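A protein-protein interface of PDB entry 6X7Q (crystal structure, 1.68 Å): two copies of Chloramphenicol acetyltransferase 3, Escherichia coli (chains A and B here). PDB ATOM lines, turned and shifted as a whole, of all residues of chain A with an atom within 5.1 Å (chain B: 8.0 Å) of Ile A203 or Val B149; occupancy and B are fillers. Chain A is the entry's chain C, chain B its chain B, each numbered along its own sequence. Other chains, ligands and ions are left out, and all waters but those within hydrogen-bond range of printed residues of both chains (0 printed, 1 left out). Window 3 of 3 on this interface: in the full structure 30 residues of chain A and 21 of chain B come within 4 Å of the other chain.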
ATOM      1  N   LEU A  32      11.852  -9.366  13.920  1.00  0.00           N
ATOM      2  CA  LEU A  32      10.793  -8.610  14.552  1.00  0.00           C
ATOM      3  C   LEU A  32      11.077  -8.525  16.046  1.00  0.00           C
ATOM      4  O   LEU A  32      11.571  -9.471  16.647  1.00  0.00           O
ATOM      5  CB  LEU A  32       9.438  -9.164  14.135  1.00  0.00           C
ATOM      6  CG  LEU A  32       8.685 -10.222  14.901  1.00  0.00           C
ATOM      7  CD1 LEU A  32       8.317  -9.816  16.326  1.00  0.00           C
ATOM      8  CD2 LEU A  32       7.371 -10.512  14.169  1.00  0.00           C
ATOM      9  N   SER A  34       9.546  -7.502  19.827  1.00  0.00           N
ATOM     10  CA  SER A  34       8.326  -7.515  20.596  1.00  0.00           C
ATOM     11  C   SER A  34       8.709  -7.371  22.077  1.00  0.00           C
ATOM     12  O   SER A  34       9.880  -7.520  22.445  1.00  0.00           O
ATOM     13  CB  SER A  34       7.595  -8.855  20.361  1.00  0.00           C
ATOM     14  OG  SER A  34       6.262  -8.724  20.780  1.00  0.00           O
ATOM     15  N   ILE A  36       8.153  -8.837  25.877  1.00  0.00           N
ATOM     16  CA  ILE A  36       7.672  -9.917  26.730  1.00  0.00           C
ATOM     17  C   ILE A  36       7.392  -9.322  28.113  1.00  0.00           C
ATOM     18  O   ILE A  36       8.245  -8.627  28.652  1.00  0.00           O
ATOM     19  CB  ILE A  36       8.711 -11.055  26.847  1.00  0.00           C
ATOM     20  CG1 ILE A  36       9.204 -11.545  25.477  1.00  0.00           C
ATOM     21  CG2 ILE A  36       8.151 -12.203  27.669  1.00  0.00           C
ATOM     22  CD1 ILE A  36       8.105 -12.190  24.679  1.00  0.00           C
ATOM     23  N   LEU A 185      12.568  -8.278  22.991  1.00  0.00           N
ATOM     24  CA  LEU A 185      13.097  -9.509  22.453  1.00  0.00           C
ATOM     25  C   LEU A 185      12.981  -9.391  20.937  1.00  0.00           C
ATOM     26  O   LEU A 185      11.876  -9.236  20.409  1.00  0.00           O
ATOM     27  CB  LEU A 185      12.292 -10.703  22.970  1.00  0.00           C
ATOM     28  CG  LEU A 185      12.820 -12.076  22.577  1.00  0.00           C
ATOM     29  CD1 LEU A 185      13.629 -12.698  23.688  1.00  0.00           C
ATOM     30  CD2 LEU A 185      11.678 -12.985  22.215  1.00  0.00           C
ATOM     31  N   VAL A 187      13.627 -11.469  17.354  1.00  0.00           N
ATOM     32  CA  VAL A 187      13.665 -12.808  16.784  1.00  0.00           C
ATOM     33  C   VAL A 187      13.952 -12.631  15.303  1.00  0.00           C
ATOM     34  O   VAL A 187      13.198 -11.937  14.622  1.00  0.00           O
ATOM     35  CB  VAL A 187      12.328 -13.536  17.013  1.00  0.00           C
ATOM     36  CG1 VAL A 187      12.391 -14.938  16.421  1.00  0.00           C
ATOM     37  CG2 VAL A 187      11.955 -13.567  18.479  1.00  0.00           C
ATOM     38  N   VAL A 199       6.762 -17.306  13.928  1.00  0.00           N
ATOM     39  CA  VAL A 199       7.485 -16.445  14.838  1.00  0.00           C
ATOM     40  C   VAL A 199       6.512 -15.961  15.927  1.00  0.00           C
ATOM     41  O   VAL A 199       6.842 -15.907  17.119  1.00  0.00           O
ATOM     42  CB  VAL A 199       8.150 -15.275  14.087  1.00  0.00           C
ATOM     43  CG1 VAL A 199       8.771 -14.285  15.046  1.00  0.00           C
ATOM     44  CG2 VAL A 199       9.207 -15.785  13.122  1.00  0.00           C
ATOM     45  N   ALA A 200       5.306 -15.576  15.524  1.00  0.00           N
ATOM     46  CA  ALA A 200       4.307 -15.177  16.516  1.00  0.00           C
ATOM     47  C   ALA A 200       4.018 -16.314  17.491  1.00  0.00           C
ATOM     48  O   ALA A 200       3.926 -16.094  18.712  1.00  0.00           O
ATOM     49  CB  ALA A 200       3.056 -14.699  15.842  1.00  0.00           C
ATOM     50  N   ARG A 201       3.859 -17.532  16.956  1.00  0.00           N
ATOM     51  CA  ARG A 201       3.600 -18.695  17.799  1.00  0.00           C
ATOM     52  C   ARG A 201       4.712 -18.907  18.824  1.00  0.00           C
ATOM     53  O   ARG A 201       4.436 -19.223  19.987  1.00  0.00           O
ATOM     54  CB  ARG A 201       3.418 -19.942  16.934  1.00  0.00           C
ATOM     55  CG  ARG A 201       3.095 -21.156  17.782  1.00  0.00           C
ATOM     56  CD  ARG A 201       2.655 -22.352  17.000  1.00  0.00           C
ATOM     57  NE  ARG A 201       3.667 -22.768  16.042  1.00  0.00           N
ATOM     58  CZ  ARG A 201       3.484 -23.801  15.218  1.00  0.00           C
ATOM     59  NH1 ARG A 201       2.302 -24.386  15.171  1.00  0.00           N
ATOM     60  NH2 ARG A 201       4.463 -24.198  14.436  1.00  0.00           N
ATOM     61  N   PHE A 202       5.981 -18.717  18.403  1.00  0.00           N
ATOM     62  CA  PHE A 202       7.125 -18.824  19.288  1.00  0.00           C
ATOM     63  C   PHE A 202       7.080 -17.754  20.388  1.00  0.00           C
ATOM     64  O   PHE A 202       7.292 -18.051  21.551  1.00  0.00           O
ATOM     65  CB  PHE A 202       8.419 -18.733  18.483  1.00  0.00           C
ATOM     66  CG  PHE A 202       9.632 -18.419  19.316  1.00  0.00           C
ATOM     67  CD1 PHE A 202      10.179 -19.356  20.176  1.00  0.00           C
ATOM     68  CD2 PHE A 202      10.134 -17.131  19.365  1.00  0.00           C
ATOM     69  CE1 PHE A 202      11.239 -19.046  21.013  1.00  0.00           C
ATOM     70  CE2 PHE A 202      11.190 -16.813  20.211  1.00  0.00           C
ATOM     71  CZ  PHE A 202      11.733 -17.759  21.062  1.00  0.00           C
ATOM     72  N   ILE A 203       6.875 -16.495  20.022  1.00  0.00           N
ATOM     73  CA  ILE A 203       6.870 -15.423  21.011  1.00  0.00           C
ATOM     74  C   ILE A 203       5.767 -15.611  22.057  1.00  0.00           C
ATOM     75  O   ILE A 203       6.018 -15.407  23.247  1.00  0.00           O
ATOM     76  CB  ILE A 203       6.746 -14.061  20.306  1.00  0.00           C
ATOM     77  CG1 ILE A 203       8.009 -13.781  19.484  1.00  0.00           C
ATOM     78  CG2 ILE A 203       6.471 -12.962  21.306  1.00  0.00           C
ATOM     79  CD1 ILE A 203       7.905 -12.649  18.551  1.00  0.00           C
ATOM     80  N   ASN A 204       4.571 -15.985  21.581  1.00  0.00           N
ATOM     81  CA  ASN A 204       3.423 -16.186  22.448  1.00  0.00           C
ATOM     82  C   ASN A 204       3.627 -17.383  23.387  1.00  0.00           C
ATOM     83  O   ASN A 204       3.210 -17.341  24.554  1.00  0.00           O
ATOM     84  CB  ASN A 204       2.160 -16.312  21.601  1.00  0.00           C
ATOM     85  CG  ASN A 204       1.728 -14.983  20.994  1.00  0.00           C
ATOM     86  OD1 ASN A 204       1.981 -13.912  21.565  1.00  0.00           O
ATOM     87  ND2 ASN A 204       1.029 -15.076  19.884  1.00  0.00           N
ATOM     88  N   ARG A 205       4.228 -18.469  22.889  1.00  0.00           N
ATOM     89  CA  ARG A 205       4.590 -19.601  23.723  1.00  0.00           C
ATOM     90  C   ARG A 205       5.621 -19.190  24.775  1.00  0.00           C
ATOM     91  O   ARG A 205       5.498 -19.572  25.936  1.00  0.00           O
ATOM     92  CB  ARG A 205       5.090 -20.780  22.877  1.00  0.00           C
ATOM     93  CG  ARG A 205       5.503 -21.974  23.718  1.00  0.00           C
ATOM     94  CD  ARG A 205       4.349 -22.477  24.558  1.00  0.00           C
ATOM     95  NE  ARG A 205       4.714 -23.680  25.299  1.00  0.00           N
ATOM     96  CZ  ARG A 205       4.200 -24.047  26.465  1.00  0.00           C
ATOM     97  NH1 ARG A 205       3.298 -23.300  27.087  1.00  0.00           N
ATOM     98  NH2 ARG A 205       4.650 -25.152  27.046  1.00  0.00           N
ATOM     99  N   LEU A 206       6.669 -18.454  24.375  1.00  0.00           N
ATOM    100  CA  LEU A 206       7.621 -17.936  25.345  1.00  0.00           C
ATOM    101  C   LEU A 206       6.919 -17.112  26.439  1.00  0.00           C
ATOM    102  O   LEU A 206       7.267 -17.216  27.648  1.00  0.00           O
ATOM    103  CB  LEU A 206       8.698 -17.099  24.654  1.00  0.00           C
ATOM    104  CG  LEU A 206       9.747 -16.487  25.590  1.00  0.00           C
ATOM    105  CD1 LEU A 206      10.513 -17.550  26.385  1.00  0.00           C
ATOM    106  CD2 LEU A 206      10.722 -15.618  24.801  1.00  0.00           C
ATOM    107  N   GLN A 207       6.043 -16.197  26.034  1.00  0.00           N
ATOM    108  CA  GLN A 207       5.270 -15.406  26.997  1.00  0.00           C
ATOM    109  C   GLN A 207       4.510 -16.321  27.982  1.00  0.00           C
ATOM    110  O   GLN A 207       4.499 -16.057  29.188  1.00  0.00           O
ATOM    111  CB  GLN A 207       4.290 -14.492  26.268  1.00  0.00           C
ATOM    112  CG  GLN A 207       3.410 -13.683  27.225  1.00  0.00           C
ATOM    113  CD  GLN A 207       4.205 -12.677  28.013  1.00  0.00           C
ATOM    114  OE1 GLN A 207       4.523 -11.594  27.511  1.00  0.00           O
ATOM    115  NE2 GLN A 207       4.598 -13.044  29.241  1.00  0.00           N
ATOM    116  N   ALA B 145      -0.284  -8.897   6.888  1.00  0.00           N
ATOM    117  CA  ALA B 145      -0.599  -8.748   8.305  1.00  0.00           C
ATOM    118  C   ALA B 145       0.025  -9.884   9.114  1.00  0.00           C
ATOM    119  O   ALA B 145       0.080 -11.018   8.628  1.00  0.00           O
ATOM    120  CB  ALA B 145      -2.096  -8.752   8.467  1.00  0.00           C
ATOM    121  N   LEU B 146       0.545  -9.554  10.297  1.00  0.00           N
ATOM    122  CA  LEU B 146       0.919 -10.538  11.320  1.00  0.00           C
ATOM    123  C   LEU B 146       0.041 -10.287  12.528  1.00  0.00           C
ATOM    124  O   LEU B 146       0.447  -9.652  13.497  1.00  0.00           O
ATOM    125  CB  LEU B 146       2.372 -10.457  11.800  1.00  0.00           C
ATOM    126  CG  LEU B 146       3.439 -10.970  10.850  1.00  0.00           C
ATOM    127  CD1 LEU B 146       3.605 -10.013   9.698  1.00  0.00           C
ATOM    128  CD2 LEU B 146       4.749 -11.130  11.603  1.00  0.00           C
ATOM    129  N   PRO B 147      -1.229 -10.710  12.483  1.00  0.00           N
ATOM    130  CA  PRO B 147      -2.173 -10.292  13.519  1.00  0.00           C
ATOM    131  C   PRO B 147      -2.048 -11.000  14.875  1.00  0.00           C
ATOM    132  O   PRO B 147      -2.710 -10.607  15.825  1.00  0.00           O
ATOM    133  CB  PRO B 147      -3.514 -10.667  12.846  1.00  0.00           C
ATOM    134  CG  PRO B 147      -3.148 -11.920  12.088  1.00  0.00           C
ATOM    135  CD  PRO B 147      -1.847 -11.538  11.431  1.00  0.00           C
ATOM    136  N   TRP B 148      -1.150 -11.986  14.983  1.00  0.00           N
ATOM    137  CA  TRP B 148      -1.043 -12.834  16.161  1.00  0.00           C
ATOM    138  C   TRP B 148      -0.077 -12.297  17.215  1.00  0.00           C
ATOM    139  O   TRP B 148      -0.079 -12.832  18.323  1.00  0.00           O
ATOM    140  CB  TRP B 148      -0.596 -14.240  15.783  1.00  0.00           C
ATOM    141  CG  TRP B 148      -1.308 -14.793  14.589  1.00  0.00           C
ATOM    142  CD1 TRP B 148      -2.548 -15.378  14.541  1.00  0.00           C
ATOM    143  CD2 TRP B 148      -0.814 -14.747  13.246  1.00  0.00           C
ATOM    144  NE1 TRP B 148      -2.848 -15.743  13.244  1.00  0.00           N
ATOM    145  CE2 TRP B 148      -1.781 -15.393  12.439  1.00  0.00           C
ATOM    146  CE3 TRP B 148       0.388 -14.308  12.663  1.00  0.00           C
ATOM    147  CZ2 TRP B 148      -1.579 -15.574  11.077  1.00  0.00           C
ATOM    148  CZ3 TRP B 148       0.564 -14.471  11.309  1.00  0.00           C
ATOM    149  CH2 TRP B 148      -0.400 -15.108  10.540  1.00  0.00           C
ATOM    150  N   VAL B 149       0.733 -11.280  16.874  1.00  0.00           N
ATOM    151  CA  VAL B 149       1.661 -10.734  17.851  1.00  0.00           C
ATOM    152  C   VAL B 149       1.874  -9.244  17.566  1.00  0.00           C
ATOM    153  O   VAL B 149       1.842  -8.806  16.424  1.00  0.00           O
ATOM    154  CB  VAL B 149       2.979 -11.539  17.829  1.00  0.00           C
ATOM    155  CG1 VAL B 149       3.791 -11.211  16.593  1.00  0.00           C
ATOM    156  CG2 VAL B 149       3.815 -11.326  19.093  1.00  0.00           C
ATOM    157  N   ASN B 150       1.988  -8.464  18.646  1.00  0.00           N
ATOM    158  CA  ASN B 150       2.322  -7.061  18.613  1.00  0.00           C
ATOM    159  C   ASN B 150       3.834  -6.972  18.422  1.00  0.00           C
ATOM    160  O   ASN B 150       4.598  -7.745  19.039  1.00  0.00           O
ATOM    161  CB  ASN B 150       1.805  -6.365  19.883  1.00  0.00           C
ATOM    162  CG  ASN B 150       2.057  -4.872  19.889  1.00  0.00           C
ATOM    163  OD1 ASN B 150       3.027  -4.434  20.513  1.00  0.00           O
ATOM    164  ND2 ASN B 150       1.273  -4.117  19.118  1.00  0.00           N
ATOM    165  N   PHE B 151       4.259  -6.130  17.497  1.00  0.00           N
ATOM    166  CA  PHE B 151       5.683  -5.856  17.358  1.00  0.00           C
ATOM    167  C   PHE B 151       5.853  -4.354  17.385  1.00  0.00           C
ATOM    168  O   PHE B 151       4.946  -3.614  16.996  1.00  0.00           O
ATOM    169  CB  PHE B 151       6.303  -6.482  16.084  1.00  0.00           C
ATOM    170  CG  PHE B 151       5.809  -6.109  14.706  1.00  0.00           C
ATOM    171  CD1 PHE B 151       5.869  -4.812  14.184  1.00  0.00           C
ATOM    172  CD2 PHE B 151       5.324  -7.096  13.865  1.00  0.00           C
ATOM    173  CE1 PHE B 151       5.401  -4.515  12.910  1.00  0.00           C
ATOM    174  CE2 PHE B 151       4.868  -6.805  12.598  1.00  0.00           C
ATOM    175  CZ  PHE B 151       4.878  -5.519  12.115  1.00  0.00           C
ATOM    176  N   ASP B 152       7.072  -3.930  17.708  1.00  0.00           N
ATOM    177  CA  ASP B 152       7.458  -2.547  17.576  1.00  0.00           C
ATOM    178  C   ASP B 152       8.388  -2.324  16.387  1.00  0.00           C
ATOM    179  O   ASP B 152       8.596  -1.172  15.999  1.00  0.00           O
ATOM    180  CB  ASP B 152       8.102  -2.063  18.871  1.00  0.00           C
ATOM    181  CG  ASP B 152       7.182  -2.258  20.067  1.00  0.00           C
ATOM    182  OD1 ASP B 152       6.125  -1.575  20.111  1.00  0.00           O
ATOM    183  OD2 ASP B 152       7.444  -3.201  20.866  1.00  0.00           O
ATOM    184  N   PHE B 154       9.794  -4.386  12.561  1.00  0.00           N
ATOM    185  CA  PHE B 154       9.808  -5.460  11.591  1.00  0.00           C
ATOM    186  C   PHE B 154      10.697  -5.024  10.431  1.00  0.00           C
ATOM    187  O   PHE B 154      10.578  -3.890   9.961  1.00  0.00           O
ATOM    188  CB  PHE B 154       8.377  -5.778  11.142  1.00  0.00           C
ATOM    189  CG  PHE B 154       8.243  -6.943  10.198  1.00  0.00           C
ATOM    190  CD1 PHE B 154       8.086  -8.228  10.678  1.00  0.00           C
ATOM    191  CD2 PHE B 154       8.347  -6.758   8.829  1.00  0.00           C
ATOM    192  CE1 PHE B 154       8.006  -9.294   9.803  1.00  0.00           C
ATOM    193  CE2 PHE B 154       8.304  -7.831   7.966  1.00  0.00           C
ATOM    194  CZ  PHE B 154       8.108  -9.097   8.459  1.00  0.00           C
ATOM    195  N   MET B 171       1.698  -5.057   8.816  1.00  0.00           N
ATOM    196  CA  MET B 171       1.082  -4.634  10.065  1.00  0.00           C
ATOM    197  C   MET B 171       1.189  -5.760  11.101  1.00  0.00           C
ATOM    198  O   MET B 171       1.345  -6.937  10.769  1.00  0.00           O
ATOM    199  CB  MET B 171      -0.371  -4.167   9.867  1.00  0.00           C
ATOM    200  CG  MET B 171      -1.335  -5.196   9.311  1.00  0.00           C
ATOM    201  SD  MET B 171      -2.870  -4.407   8.653  1.00  0.00           S
ATOM    202  CE  MET B 171      -2.432  -4.172   6.928  1.00  0.00           C
ATOM    203  N   ALA B 172       1.230  -5.349  12.370  1.00  0.00           N
ATOM    204  CA  ALA B 172       1.222  -6.239  13.533  1.00  0.00           C
ATOM    205  C   ALA B 172      -0.171  -6.257  14.179  1.00  0.00           C
ATOM    206  O   ALA B 172      -1.080  -5.553  13.758  1.00  0.00           O
ATOM    207  CB  ALA B 172       2.215  -5.749  14.533  1.00  0.00           C
ATOM    208  N   LYS B 173      -0.322  -7.050  15.217  1.00  0.00           N
ATOM    209  CA  LYS B 173      -1.490  -7.004  16.095  1.00  0.00           C
ATOM    210  C   LYS B 173      -1.645  -5.620  16.729  1.00  0.00           C
ATOM    211  O   LYS B 173      -0.701  -5.109  17.325  1.00  0.00           O
ATOM    212  CB  LYS B 173      -1.315  -8.039  17.209  1.00  0.00           C
ATOM    213  CG  LYS B 173      -2.523  -8.175  18.128  1.00  0.00           C
ATOM    214  CD  LYS B 173      -2.330  -9.295  19.109  1.00  0.00           C
ATOM    215  CE  LYS B 173      -3.575  -9.511  19.943  1.00  0.00           C
ATOM    216  NZ  LYS B 173      -3.355 -10.577  20.952  1.00  0.00           N
ATOM    217  N   TYR B 174      -2.846  -5.001  16.601  1.00  0.00           N
ATOM    218  CA  TYR B 174      -3.091  -3.728  17.255  1.00  0.00           C
ATOM    219  C   TYR B 174      -3.235  -3.945  18.756  1.00  0.00           C
ATOM    220  O   TYR B 174      -3.561  -5.039  19.228  1.00  0.00           O
ATOM    221  CB  TYR B 174      -4.252  -2.952  16.620  1.00  0.00           C
ATOM    222  CG  TYR B 174      -5.562  -3.671  16.483  1.00  0.00           C
ATOM    223  CD1 TYR B 174      -6.239  -4.173  17.581  1.00  0.00           C
ATOM    224  CD2 TYR B 174      -6.138  -3.867  15.228  1.00  0.00           C
ATOM    225  CE1 TYR B 174      -7.466  -4.819  17.441  1.00  0.00           C
ATOM    226  CE2 TYR B 174      -7.361  -4.505  15.073  1.00  0.00           C
ATOM    227  CZ  TYR B 174      -8.039  -4.974  16.186  1.00  0.00           C
ATOM    228  OH  TYR B 174      -9.243  -5.675  16.045  1.00  0.00           O
ATOM    229  N   GLN B 175      -2.952  -2.896  19.516  1.00  0.00           N
ATOM    230  CA  GLN B 175      -3.147  -2.946  20.956  1.00  0.00           C
ATOM    231  C   GLN B 175      -3.343  -1.542  21.502  1.00  0.00           C
ATOM    232  O   GLN B 175      -2.877  -0.537  20.962  1.00  0.00           O
ATOM    233  CB  GLN B 175      -2.094  -3.771  21.696  1.00  0.00           C
ATOM    234  CG  GLN B 175      -0.750  -3.145  21.944  1.00  0.00           C
ATOM    235  CD  GLN B 175       0.156  -4.060  22.772  1.00  0.00           C
ATOM    236  OE1 GLN B 175       0.969  -3.599  23.570  1.00  0.00           O
ATOM    237  NE2 GLN B 175       0.042  -5.363  22.595  1.00  0.00           N
ATOM    238  N   PRO B 184       0.816  -1.160  14.812  1.00  0.00           N
ATOM    239  CA  PRO B 184       2.187  -1.060  14.303  1.00  0.00           C
ATOM    240  C   PRO B 184       2.205  -1.341  12.808  1.00  0.00           C
ATOM    241  O   PRO B 184       1.584  -2.288  12.333  1.00  0.00           O
ATOM    242  CB  PRO B 184       2.954  -2.133  15.080  1.00  0.00           C
ATOM    243  CG  PRO B 184       2.052  -2.435  16.280  1.00  0.00           C
ATOM    244  CD  PRO B 184       0.645  -2.296  15.730  1.00  0.00           C
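O of Trp B148 is in hydrogen-bond range of ND2 of Asn A204, at 2.9 Å.
The backbone carbonyl oxygen (O) of Asn B150 sits at hydrogen-bond distance from the side-chain hydroxyl (OG) of Ser A34 (2.6 Å).
O of Met B171 sits at hydrogen-bond distance from N of Leu B146.
The backbone NH (N) of Lys B173 is in hydrogen-bond range of the backbone carbonyl oxygen (O) of Leu B146 (3.2 Å).
The side-chain amide nitrogen (ND2) of Asn B150 lies within hydrogen-bond range of the backbone carbonyl oxygen (O) of Lys B173, 2.8 Å away.
The backbone carbonyl oxygen (O) of Leu A32 is in hydrogen-bond range of the backbone NH (N) of Val A187 (3.0 Å).
N of Leu A185 is in hydrogen-bond range of O of Ser A34 (2.8 Å).
The side-chain amide nitrogen of Asn A204 lies within hydrogen-bond range of the backbone carbonyl oxygen of Ala A200, 3.3 Å away.
Leu A32 touches Leu B146 (CD2 to CD2, 3.7 Å).
Phe B151 touches Leu A32.
Leu A32 touches Phe B154.
Ser A34 touches Val B149.
CB of Ala A200 touches CB of Trp B148 (3.7 Å).
CB of Ala A200 touches CG1 of Val B149, at 3.6 Å.
CG2 of Val B149 touches CG2 of Ile A203, at 3.8 Å.
Printed residues of chain B within 4 Å of Ile A203: Val B149 (3.8 Å).
Of the printed residues of chain A, Leu B146 touches Leu A32 (3.7 Å).
Val B149 touches just these residues of chain A: Ser A34, Ala A200 and Ile A203.
Of the printed residues of chain A, Asn B150 touches Ser A34.
Of the printed residues of chain A, Phe B151 touches Leu A32.
The nearest residue of chain A that does not touch Val B149 is Asn A204 (4.02 Å).
The nearest printed residue of chain A that does not touch Trp B148 is Arg A201 (5.7 Å).
Of the 14 printed residues of chain A, 5 touch a printed residue of chain B.
Hydrophobic or aromatic side chains of chain A that line the printed part of chain B: Leu A32, Ala A200 and Ile A203.
Of the 15 printed residues of chain B, 6 touch a printed residue of chain A.
Printed residues of chain B that touch a printed residue of chain A: Leu B146, Trp B148, Val B149, Asn B150, Phe B151 and Phe B154.
Hydrophobic or aromatic side chains of chain B that line the printed part of chain A: Leu B146, Trp B148, Val B149, Phe B151 and Phe B154.
Among the printed residues, 9 pairs touch across the chains.
Among the printed residues, no Asp or Glu carboxylate lies within 4 Å of a Lys or Arg side-chain nitrogen of the other chain.
No position is printed for both chains.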
